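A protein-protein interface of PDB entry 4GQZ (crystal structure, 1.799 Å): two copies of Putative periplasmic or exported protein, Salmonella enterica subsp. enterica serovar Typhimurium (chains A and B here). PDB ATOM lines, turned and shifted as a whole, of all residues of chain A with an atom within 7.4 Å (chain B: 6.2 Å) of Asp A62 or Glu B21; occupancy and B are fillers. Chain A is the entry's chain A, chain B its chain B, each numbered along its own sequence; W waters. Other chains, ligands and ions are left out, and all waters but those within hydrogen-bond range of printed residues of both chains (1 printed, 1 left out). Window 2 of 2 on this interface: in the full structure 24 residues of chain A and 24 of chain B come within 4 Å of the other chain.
The side-chain carboxylate (OE2) of Glu A21 sits at hydrogen-bond distance from the backbone NH (N) of Asp B62.
The backbone NH (N) of Val B20 is in hydrogen-bond range of the backbone carbonyl oxygen (O) of Leu A60, 2.9 Å away.
The side-chain carboxylate of Asp A62 sits close to the side-chain carboxylate of Glu B21.
NH2 of Arg A126 sits at hydrogen-bond distance from O of Gly A61 (3.0 Å).
The backbone carbonyl oxygen (O) of Lys A63 is in hydrogen-bond range of the guanidinium group (NH2) of Arg A126.
The side-chain amino group (NZ) of Lys B18 is in hydrogen-bond range of the side-chain hydroxyl (OG1) of Thr B26 (3.3 Å).
The backbone NH (N) of Thr B19 is in hydrogen-bond range of the side-chain amide oxygen (OE1) of Gln B22, 2.9 Å away.
Among the printed residues, merely in contact across the chains: Leu A60 with Thr B19 (3.3 Å), Glu A21 with Gly B61 (3.3 Å), Gly A61 with Thr B19 (3.4 Å), Pro A59 with Lys B18 (3.5 Å), Pro A59 with Ile B23 (3.6 Å), Arg A126 with Thr B19 (3.8 Å) and Pro A59 with Val B20 (3.8 Å).
Of the printed residues of chain B, Asp A62 touches Glu B21.
Of the printed residues of chain A, Glu B21 touches Asp A62 (2.6 Å).
Of the printed residues of chain A, Asp B62 touches Glu A21 (3.1 Å).
Of the printed residues of chain A, Ile B23 touches Pro A59 (3.6 Å).
Of the printed residues of chain A, Val B20 touches Pro A59 and Leu A60.
Phe A64 touches none of the printed residues of chain B.
The nearest printed residue of chain B that does not touch Gly A61 is Val B20 (4.1 Å).
Of the 13 printed residues of chain B, 7 touch a printed residue of chain A.
Hydrophobic or aromatic side chains of chain B that line the printed part of chain A: Val B20 and Ile B23.
Hydrophobic or aromatic side chains of chain A that line the printed part of chain B: Pro A59.
Among the printed residues, 10 pairs touch across the chains.
Among the printed residues, no Asp or Glu carboxylate lies within 4 Å of a Lys or Arg side-chain nitrogen of the other chain.
Glu A21 touches Gly B61, but with the chains exchanged Gly A61 does not touch Glu B21 (5.3 Å).
Glu A21 touches Asp B62, and with the chains exchanged Asp A62 touches Glu B21.
6 positions are printed for both chains.
Of the 10 pairs that touch across the chains among the printed residues, 2 have their exchanged pair printed and touching as well.
Water W1 lies within hydrogen-bond range of the backbone NH of Asp B62, the backbone NH of Asp A62 and the side-chain carboxylate of Glu A21.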
ATOM      1  N   VAL A  20     -23.252  29.238 -23.387  1.00  0.00           N
ATOM      2  CA  VAL A  20     -22.424  28.090 -23.760  1.00  0.00           C
ATOM      3  C   VAL A  20     -23.041  27.253 -24.891  1.00  0.00           C
ATOM      4  O   VAL A  20     -22.310  26.683 -25.705  1.00  0.00           O
ATOM      5  CB  VAL A  20     -22.007  27.235 -22.512  1.00  0.00           C
ATOM      6  CG1 VAL A  20     -23.187  26.460 -21.971  1.00  0.00           C
ATOM      7  CG2 VAL A  20     -20.847  26.282 -22.859  1.00  0.00           C
ATOM      8  N   GLU A  21     -24.369  27.202 -24.982  1.00  0.00           N
ATOM      9  CA  GLU A  21     -25.022  26.497 -26.099  1.00  0.00           C
ATOM     10  C   GLU A  21     -24.783  27.196 -27.439  1.00  0.00           C
ATOM     11  O   GLU A  21     -24.549  26.540 -28.448  1.00  0.00           O
ATOM     12  CB  GLU A  21     -26.538  26.346 -25.891  1.00  0.00           C
ATOM     13  CG  GLU A  21     -26.978  25.223 -24.919  1.00  0.00           C
ATOM     14  CD  GLU A  21     -27.093  25.669 -23.461  1.00  0.00           C
ATOM     15  OE1 GLU A  21     -27.543  24.835 -22.629  1.00  0.00           O
ATOM     16  OE2 GLU A  21     -26.753  26.841 -23.134  1.00  0.00           O
ATOM     17  N   PRO A  59     -17.598  24.999 -18.673  1.00  0.00           N
ATOM     18  CA  PRO A  59     -18.656  24.118 -18.185  1.00  0.00           C
ATOM     19  C   PRO A  59     -19.905  24.216 -19.048  1.00  0.00           C
ATOM     20  O   PRO A  59     -20.340  25.314 -19.406  1.00  0.00           O
ATOM     21  CB  PRO A  59     -18.948  24.681 -16.792  1.00  0.00           C
ATOM     22  CG  PRO A  59     -17.621  25.235 -16.357  1.00  0.00           C
ATOM     23  CD  PRO A  59     -17.070  25.866 -17.601  1.00  0.00           C
ATOM     24  N   LEU A  60     -20.473  23.070 -19.390  1.00  0.00           N
ATOM     25  CA  LEU A  60     -21.764  23.056 -20.058  1.00  0.00           C
ATOM     26  C   LEU A  60     -22.864  23.362 -19.048  1.00  0.00           C
ATOM     27  O   LEU A  60     -22.604  23.485 -17.849  1.00  0.00           O
ATOM     28  CB  LEU A  60     -22.003  21.692 -20.690  1.00  0.00           C
ATOM     29  CG  LEU A  60     -21.660  21.482 -22.166  1.00  0.00           C
ATOM     30  CD1 LEU A  60     -20.664  22.470 -22.680  1.00  0.00           C
ATOM     31  CD2 LEU A  60     -21.183  20.056 -22.377  1.00  0.00           C
ATOM     32  N   GLY A  61     -24.093  23.481 -19.543  1.00  0.00           N
ATOM     33  CA  GLY A  61     -25.247  23.778 -18.706  1.00  0.00           C
ATOM     34  C   GLY A  61     -26.044  22.521 -18.412  1.00  0.00           C
ATOM     35  O   GLY A  61     -25.481  21.420 -18.369  1.00  0.00           O
ATOM     36  N   ASP A  62     -27.352  22.693 -18.244  1.00  0.00           N
ATOM     37  CA  ASP A  62     -28.259  21.643 -17.796  1.00  0.00           C
ATOM     38  C   ASP A  62     -28.492  20.558 -18.818  1.00  0.00           C
ATOM     39  O   ASP A  62     -29.082  19.519 -18.492  1.00  0.00           O
ATOM     40  CB  ASP A  62     -29.641  22.240 -17.516  1.00  0.00           C
ATOM     41  CG  ASP A  62     -29.689  23.062 -16.273  1.00  0.00           C
ATOM     42  OD1 ASP A  62     -28.861  22.855 -15.365  1.00  0.00           O
ATOM     43  OD2 ASP A  62     -30.615  23.900 -16.195  1.00  0.00           O
ATOM     44  N   LYS A  63     -28.108  20.812 -20.067  1.00  0.00           N
ATOM     45  CA  LYS A  63     -28.354  19.846 -21.130  1.00  0.00           C
ATOM     46  C   LYS A  63     -27.090  19.234 -21.723  1.00  0.00           C
ATOM     47  O   LYS A  63     -26.058  19.905 -21.897  1.00  0.00           O
ATOM     48  CB  LYS A  63     -29.248  20.456 -22.213  1.00  0.00           C
ATOM     49  CG  LYS A  63     -30.730  20.528 -21.768  1.00  0.00           C
ATOM     50  CD  LYS A  63     -31.577  21.169 -22.831  1.00  0.00           C
ATOM     51  CE  LYS A  63     -32.999  21.386 -22.321  1.00  0.00           C
ATOM     52  NZ  LYS A  63     -33.620  20.098 -21.876  1.00  0.00           N
ATOM     53  N   PHE A  64     -27.186  17.938 -21.995  1.00  0.00           N
ATOM     54  CA  PHE A  64     -26.141  17.160 -22.658  1.00  0.00           C
ATOM     55  C   PHE A  64     -26.148  17.445 -24.159  1.00  0.00           C
ATOM     56  O   PHE A  64     -27.213  17.465 -24.786  1.00  0.00           O
ATOM     57  CB  PHE A  64     -26.475  15.682 -22.422  1.00  0.00           C
ATOM     58  CG  PHE A  64     -25.400  14.727 -22.845  1.00  0.00           C
ATOM     59  CD1 PHE A  64     -25.288  14.319 -24.172  1.00  0.00           C
ATOM     60  CD2 PHE A  64     -24.523  14.203 -21.904  1.00  0.00           C
ATOM     61  CE1 PHE A  64     -24.287  13.429 -24.557  1.00  0.00           C
ATOM     62  CE2 PHE A  64     -23.536  13.322 -22.279  1.00  0.00           C
ATOM     63  CZ  PHE A  64     -23.412  12.932 -23.606  1.00  0.00           C
ATOM     64  N   TRP A 123     -29.492  18.867 -28.140  1.00  0.00           N
ATOM     65  CA  TRP A 123     -29.399  19.147 -26.712  1.00  0.00           C
ATOM     66  C   TRP A 123     -30.452  18.350 -25.963  1.00  0.00           C
ATOM     67  O   TRP A 123     -31.651  18.474 -26.227  1.00  0.00           O
ATOM     68  CB  TRP A 123     -29.601  20.627 -26.451  1.00  0.00           C
ATOM     69  CG  TRP A 123     -28.505  21.444 -27.037  1.00  0.00           C
ATOM     70  CD1 TRP A 123     -28.519  22.088 -28.242  1.00  0.00           C
ATOM     71  CD2 TRP A 123     -27.220  21.703 -26.453  1.00  0.00           C
ATOM     72  NE1 TRP A 123     -27.318  22.739 -28.438  1.00  0.00           N
ATOM     73  CE2 TRP A 123     -26.509  22.525 -27.348  1.00  0.00           C
ATOM     74  CE3 TRP A 123     -26.602  21.326 -25.250  1.00  0.00           C
ATOM     75  CZ2 TRP A 123     -25.199  22.956 -27.096  1.00  0.00           C
ATOM     76  CZ3 TRP A 123     -25.314  21.763 -24.995  1.00  0.00           C
ATOM     77  CH2 TRP A 123     -24.624  22.566 -25.920  1.00  0.00           C
ATOM     78  N   LEU A 124     -29.999  17.547 -25.010  1.00  0.00           N
ATOM     79  CA  LEU A 124     -30.852  16.568 -24.343  1.00  0.00           C
ATOM     80  C   LEU A 124     -30.809  16.716 -22.831  1.00  0.00           C
ATOM     81  O   LEU A 124     -29.817  17.209 -22.273  1.00  0.00           O
ATOM     82  CB  LEU A 124     -30.397  15.157 -24.738  1.00  0.00           C
ATOM     83  CG  LEU A 124     -30.403  14.855 -26.241  1.00  0.00           C
ATOM     84  CD1 LEU A 124     -29.736  13.508 -26.543  1.00  0.00           C
ATOM     85  CD2 LEU A 124     -31.830  14.872 -26.752  1.00  0.00           C
ATOM     86  N   PRO A 125     -31.896  16.310 -22.154  1.00  0.00           N
ATOM     87  CA  PRO A 125     -31.877  16.236 -20.690  1.00  0.00           C
ATOM     88  C   PRO A 125     -30.797  15.255 -20.225  1.00  0.00           C
ATOM     89  O   PRO A 125     -30.541  14.250 -20.912  1.00  0.00           O
ATOM     90  CB  PRO A 125     -33.274  15.699 -20.335  1.00  0.00           C
ATOM     91  CG  PRO A 125     -33.825  15.100 -21.624  1.00  0.00           C
ATOM     92  CD  PRO A 125     -33.205  15.934 -22.721  1.00  0.00           C
ATOM     93  N   ARG A 126     -30.180  15.553 -19.083  1.00  0.00           N
ATOM     94  CA  ARG A 126     -29.076  14.764 -18.548  1.00  0.00           C
ATOM     95  C   ARG A 126     -29.610  13.568 -17.791  1.00  0.00           C
ATOM     96  O   ARG A 126     -30.754  13.582 -17.341  1.00  0.00           O
ATOM     97  CB  ARG A 126     -28.221  15.620 -17.602  1.00  0.00           C
ATOM     98  CG  ARG A 126     -27.504  16.769 -18.284  1.00  0.00           C
ATOM     99  CD  ARG A 126     -26.455  17.404 -17.367  1.00  0.00           C
ATOM    100  NE  ARG A 126     -25.686  18.395 -18.111  1.00  0.00           N
ATOM    101  CZ  ARG A 126     -24.592  18.101 -18.811  1.00  0.00           C
ATOM    102  NH1 ARG A 126     -24.135  16.849 -18.839  1.00  0.00           N
ATOM    103  NH2 ARG A 126     -23.949  19.056 -19.472  1.00  0.00           N
ATOM    104  N   ASN A 127     -28.781  12.537 -17.661  1.00  0.00           N
ATOM    105  CA  ASN A 127     -29.152  11.324 -16.939  1.00  0.00           C
ATOM    106  C   ASN A 127     -30.447  10.705 -17.425  1.00  0.00           C
ATOM    107  O   ASN A 127     -31.303  10.313 -16.637  1.00  0.00           O
ATOM    108  CB  ASN A 127     -29.200  11.591 -15.439  1.00  0.00           C
ATOM    109  CG  ASN A 127     -27.917  12.203 -14.948  1.00  0.00           C
ATOM    110  OD1 ASN A 127     -27.877  13.376 -14.597  1.00  0.00           O
ATOM    111  ND2 ASN A 127     -26.843  11.428 -14.985  1.00  0.00           N
ATOM    112  N   LYS B  18     -18.387  20.291 -12.665  1.00  0.00           N
ATOM    113  CA  LYS B  18     -19.751  20.781 -12.443  1.00  0.00           C
ATOM    114  C   LYS B  18     -20.316  21.503 -13.665  1.00  0.00           C
ATOM    115  O   LYS B  18     -19.575  22.135 -14.419  1.00  0.00           O
ATOM    116  CB  LYS B  18     -19.782  21.759 -11.262  1.00  0.00           C
ATOM    117  CG  LYS B  18     -19.590  21.152  -9.874  1.00  0.00           C
ATOM    118  CD  LYS B  18     -19.473  22.273  -8.840  1.00  0.00           C
ATOM    119  CE  LYS B  18     -19.274  21.744  -7.422  1.00  0.00           C
ATOM    120  NZ  LYS B  18     -20.536  21.210  -6.830  1.00  0.00           N
ATOM    121  N   THR B  19     -21.632  21.436 -13.846  1.00  0.00           N
ATOM    122  CA  THR B  19     -22.293  22.283 -14.837  1.00  0.00           C
ATOM    123  C   THR B  19     -22.205  23.726 -14.362  1.00  0.00           C
ATOM    124  O   THR B  19     -21.901  23.987 -13.187  1.00  0.00           O
ATOM    125  CB  THR B  19     -23.783  21.944 -15.032  1.00  0.00           C
ATOM    126  OG1 THR B  19     -24.511  22.254 -13.839  1.00  0.00           O
ATOM    127  CG2 THR B  19     -23.982  20.485 -15.410  1.00  0.00           C
ATOM    128  N   VAL B  20     -22.454  24.670 -15.258  1.00  0.00           N
ATOM    129  CA  VAL B  20     -22.306  26.062 -14.858  1.00  0.00           C
ATOM    130  C   VAL B  20     -23.348  26.456 -13.789  1.00  0.00           C
ATOM    131  O   VAL B  20     -23.040  27.231 -12.865  1.00  0.00           O
ATOM    132  CB  VAL B  20     -22.225  27.014 -16.087  1.00  0.00           C
ATOM    133  CG1 VAL B  20     -23.527  27.025 -16.857  1.00  0.00           C
ATOM    134  CG2 VAL B  20     -21.805  28.410 -15.666  1.00  0.00           C
ATOM    135  N   GLU B  21     -24.551  25.890 -13.874  1.00  0.00           N
ATOM    136  CA  GLU B  21     -25.573  26.102 -12.847  1.00  0.00           C
ATOM    137  C   GLU B  21     -25.138  25.589 -11.474  1.00  0.00           C
ATOM    138  O   GLU B  21     -25.358  26.251 -10.454  1.00  0.00           O
ATOM    139  CB  GLU B  21     -26.898  25.435 -13.227  1.00  0.00           C
ATOM    140  CG  GLU B  21     -27.608  26.074 -14.406  1.00  0.00           C
ATOM    141  CD  GLU B  21     -29.110  25.803 -14.414  1.00  0.00           C
ATOM    142  OE1 GLU B  21     -29.634  25.175 -13.455  1.00  0.00           O
ATOM    143  OE2 GLU B  21     -29.778  26.234 -15.393  1.00  0.00           O
ATOM    144  N   GLN B  22     -24.552  24.396 -11.446  1.00  0.00           N
ATOM    145  CA  GLN B  22     -24.041  23.835 -10.202  1.00  0.00           C
ATOM    146  C   GLN B  22     -22.932  24.711  -9.630  1.00  0.00           C
ATOM    147  O   GLN B  22     -22.813  24.844  -8.416  1.00  0.00           O
ATOM    148  CB  GLN B  22     -23.542  22.395 -10.413  1.00  0.00           C
ATOM    149  CG  GLN B  22     -24.632  21.426 -10.875  1.00  0.00           C
ATOM    150  CD  GLN B  22     -24.095  20.049 -11.290  1.00  0.00           C
ATOM    151  OE1 GLN B  22     -22.962  19.914 -11.758  1.00  0.00           O
ATOM    152  NE2 GLN B  22     -24.919  19.024 -11.112  1.00  0.00           N
ATOM    153  N   ILE B  23     -22.123  25.319 -10.493  1.00  0.00           N
ATOM    154  CA  ILE B  23     -21.054  26.206 -10.002  1.00  0.00           C
ATOM    155  C   ILE B  23     -21.657  27.459  -9.367  1.00  0.00           C
ATOM    156  O   ILE B  23     -21.304  27.829  -8.244  1.00  0.00           O
ATOM    157  CB  ILE B  23     -20.104  26.654 -11.121  1.00  0.00           C
ATOM    158  CG1 ILE B  23     -19.338  25.460 -11.689  1.00  0.00           C
ATOM    159  CG2 ILE B  23     -19.119  27.699 -10.611  1.00  0.00           C
ATOM    160  CD1 ILE B  23     -18.506  25.809 -12.915  1.00  0.00           C
ATOM    161  N   VAL B  24     -22.544  28.124 -10.107  1.00  0.00           N
ATOM    162  CA  VAL B  24     -23.236  29.310  -9.603  1.00  0.00           C
ATOM    163  C   VAL B  24     -23.980  29.008  -8.309  1.00  0.00           C
ATOM    164  O   VAL B  24     -23.791  29.723  -7.297  1.00  0.00           O
ATOM    165  CB  VAL B  24     -24.167  29.896 -10.680  1.00  0.00           C
ATOM    166  CG1 VAL B  24     -25.049  31.000 -10.104  1.00  0.00           C
ATOM    167  CG2 VAL B  24     -23.331  30.426 -11.840  1.00  0.00           C
ATOM    168  N   ASP B  25     -24.792  27.944  -8.313  1.00  0.00           N
ATOM    169  CA  ASP B  25     -25.496  27.516  -7.099  1.00  0.00           C
ATOM    170  C   ASP B  25     -24.531  27.270  -5.933  1.00  0.00           C
ATOM    171  O   ASP B  25     -24.799  27.666  -4.802  1.00  0.00           O
ATOM    172  CB  ASP B  25     -26.285  26.223  -7.342  1.00  0.00           C
ATOM    173  CG  ASP B  25     -27.453  26.411  -8.282  1.00  0.00           C
ATOM    174  OD1 ASP B  25     -27.800  27.572  -8.577  1.00  0.00           O
ATOM    175  OD2 ASP B  25     -28.023  25.387  -8.732  1.00  0.00           O
ATOM    176  N   THR B  26     -23.418  26.597  -6.204  1.00  0.00           N
ATOM    177  CA  THR B  26     -22.481  26.254  -5.132  1.00  0.00           C
ATOM    178  C   THR B  26     -21.919  27.520  -4.504  1.00  0.00           C
ATOM    179  O   THR B  26     -21.842  27.652  -3.266  1.00  0.00           O
ATOM    180  CB  THR B  26     -21.305  25.392  -5.657  1.00  0.00           C
ATOM    181  OG1 THR B  26     -21.816  24.183  -6.256  1.00  0.00           O
ATOM    182  CG2 THR B  26     -20.353  25.045  -4.532  1.00  0.00           C
ATOM    183  N   GLY B  61     -25.734  29.263 -19.380  1.00  0.00           N
ATOM    184  CA  GLY B  61     -26.485  28.415 -20.280  1.00  0.00           C
ATOM    185  C   GLY B  61     -27.807  29.032 -20.691  1.00  0.00           C
ATOM    186  O   GLY B  61     -27.920  30.254 -20.767  1.00  0.00           O
ATOM    187  N   ASP B  62     -28.794  28.179 -20.960  1.00  0.00           N
ATOM    188  CA  ASP B  62     -30.093  28.594 -21.508  1.00  0.00           C
ATOM    189  C   ASP B  62     -30.913  29.433 -20.528  1.00  0.00           C
ATOM    190  O   ASP B  62     -31.850  30.138 -20.927  1.00  0.00           O
ATOM    191  CB  ASP B  62     -30.936  27.363 -21.857  1.00  0.00           C
ATOM    192  CG  ASP B  62     -30.477  26.659 -23.116  1.00  0.00           C
ATOM    193  OD1 ASP B  62     -29.723  27.260 -23.918  1.00  0.00           O
ATOM    194  OD2 ASP B  62     -30.909  25.496 -23.309  1.00  0.00           O
ATOM    195  N   LYS B  63     -30.583  29.335 -19.247  1.00  0.00           N
ATOM    196  CA  LYS B  63     -31.364  30.001 -18.213  1.00  0.00           C
ATOM    197  C   LYS B  63     -30.676  31.242 -17.659  1.00  0.00           C
ATOM    198  O   LYS B  63     -29.451  31.269 -17.482  1.00  0.00           O
ATOM    199  CB  LYS B  63     -31.627  29.035 -17.061  1.00  0.00           C
ATOM    200  CG  LYS B  63     -32.434  27.812 -17.455  1.00  0.00           C
ATOM    201  CD  LYS B  63     -33.855  28.216 -17.787  1.00  0.00           C
ATOM    202  CE  LYS B  63     -34.728  26.990 -18.069  1.00  0.00           C
ATOM    203  NZ  LYS B  63     -34.077  26.088 -19.064  1.00  0.00           N
ATOM    204  N   TRP B 123     -33.553  30.211 -11.508  1.00  0.00           N
ATOM    205  CA  TRP B 123     -33.161  30.060 -12.898  1.00  0.00           C
ATOM    206  C   TRP B 123     -34.383  30.224 -13.786  1.00  0.00           C
ATOM    207  O   TRP B 123     -35.363  29.478 -13.672  1.00  0.00           O
ATOM    208  CB  TRP B 123     -32.512  28.694 -13.102  1.00  0.00           C
ATOM    209  CG  TRP B 123     -31.169  28.565 -12.404  1.00  0.00           C
ATOM    210  CD1 TRP B 123     -30.923  27.996 -11.177  1.00  0.00           C
ATOM    211  CD2 TRP B 123     -29.901  29.009 -12.901  1.00  0.00           C
ATOM    212  NE1 TRP B 123     -29.580  28.064 -10.890  1.00  0.00           N
ATOM    213  CE2 TRP B 123     -28.930  28.673 -11.932  1.00  0.00           C
ATOM    214  CE3 TRP B 123     -29.494  29.660 -14.068  1.00  0.00           C
ATOM    215  CZ2 TRP B 123     -27.576  28.977 -12.094  1.00  0.00           C
ATOM    216  CZ3 TRP B 123     -28.154  29.954 -14.233  1.00  0.00           C
ATOM    217  CH2 TRP B 123     -27.207  29.617 -13.246  1.00  0.00           C
HETATM  218  O   HOH W   1     -28.610  25.348 -19.566  1.00  0.00           O
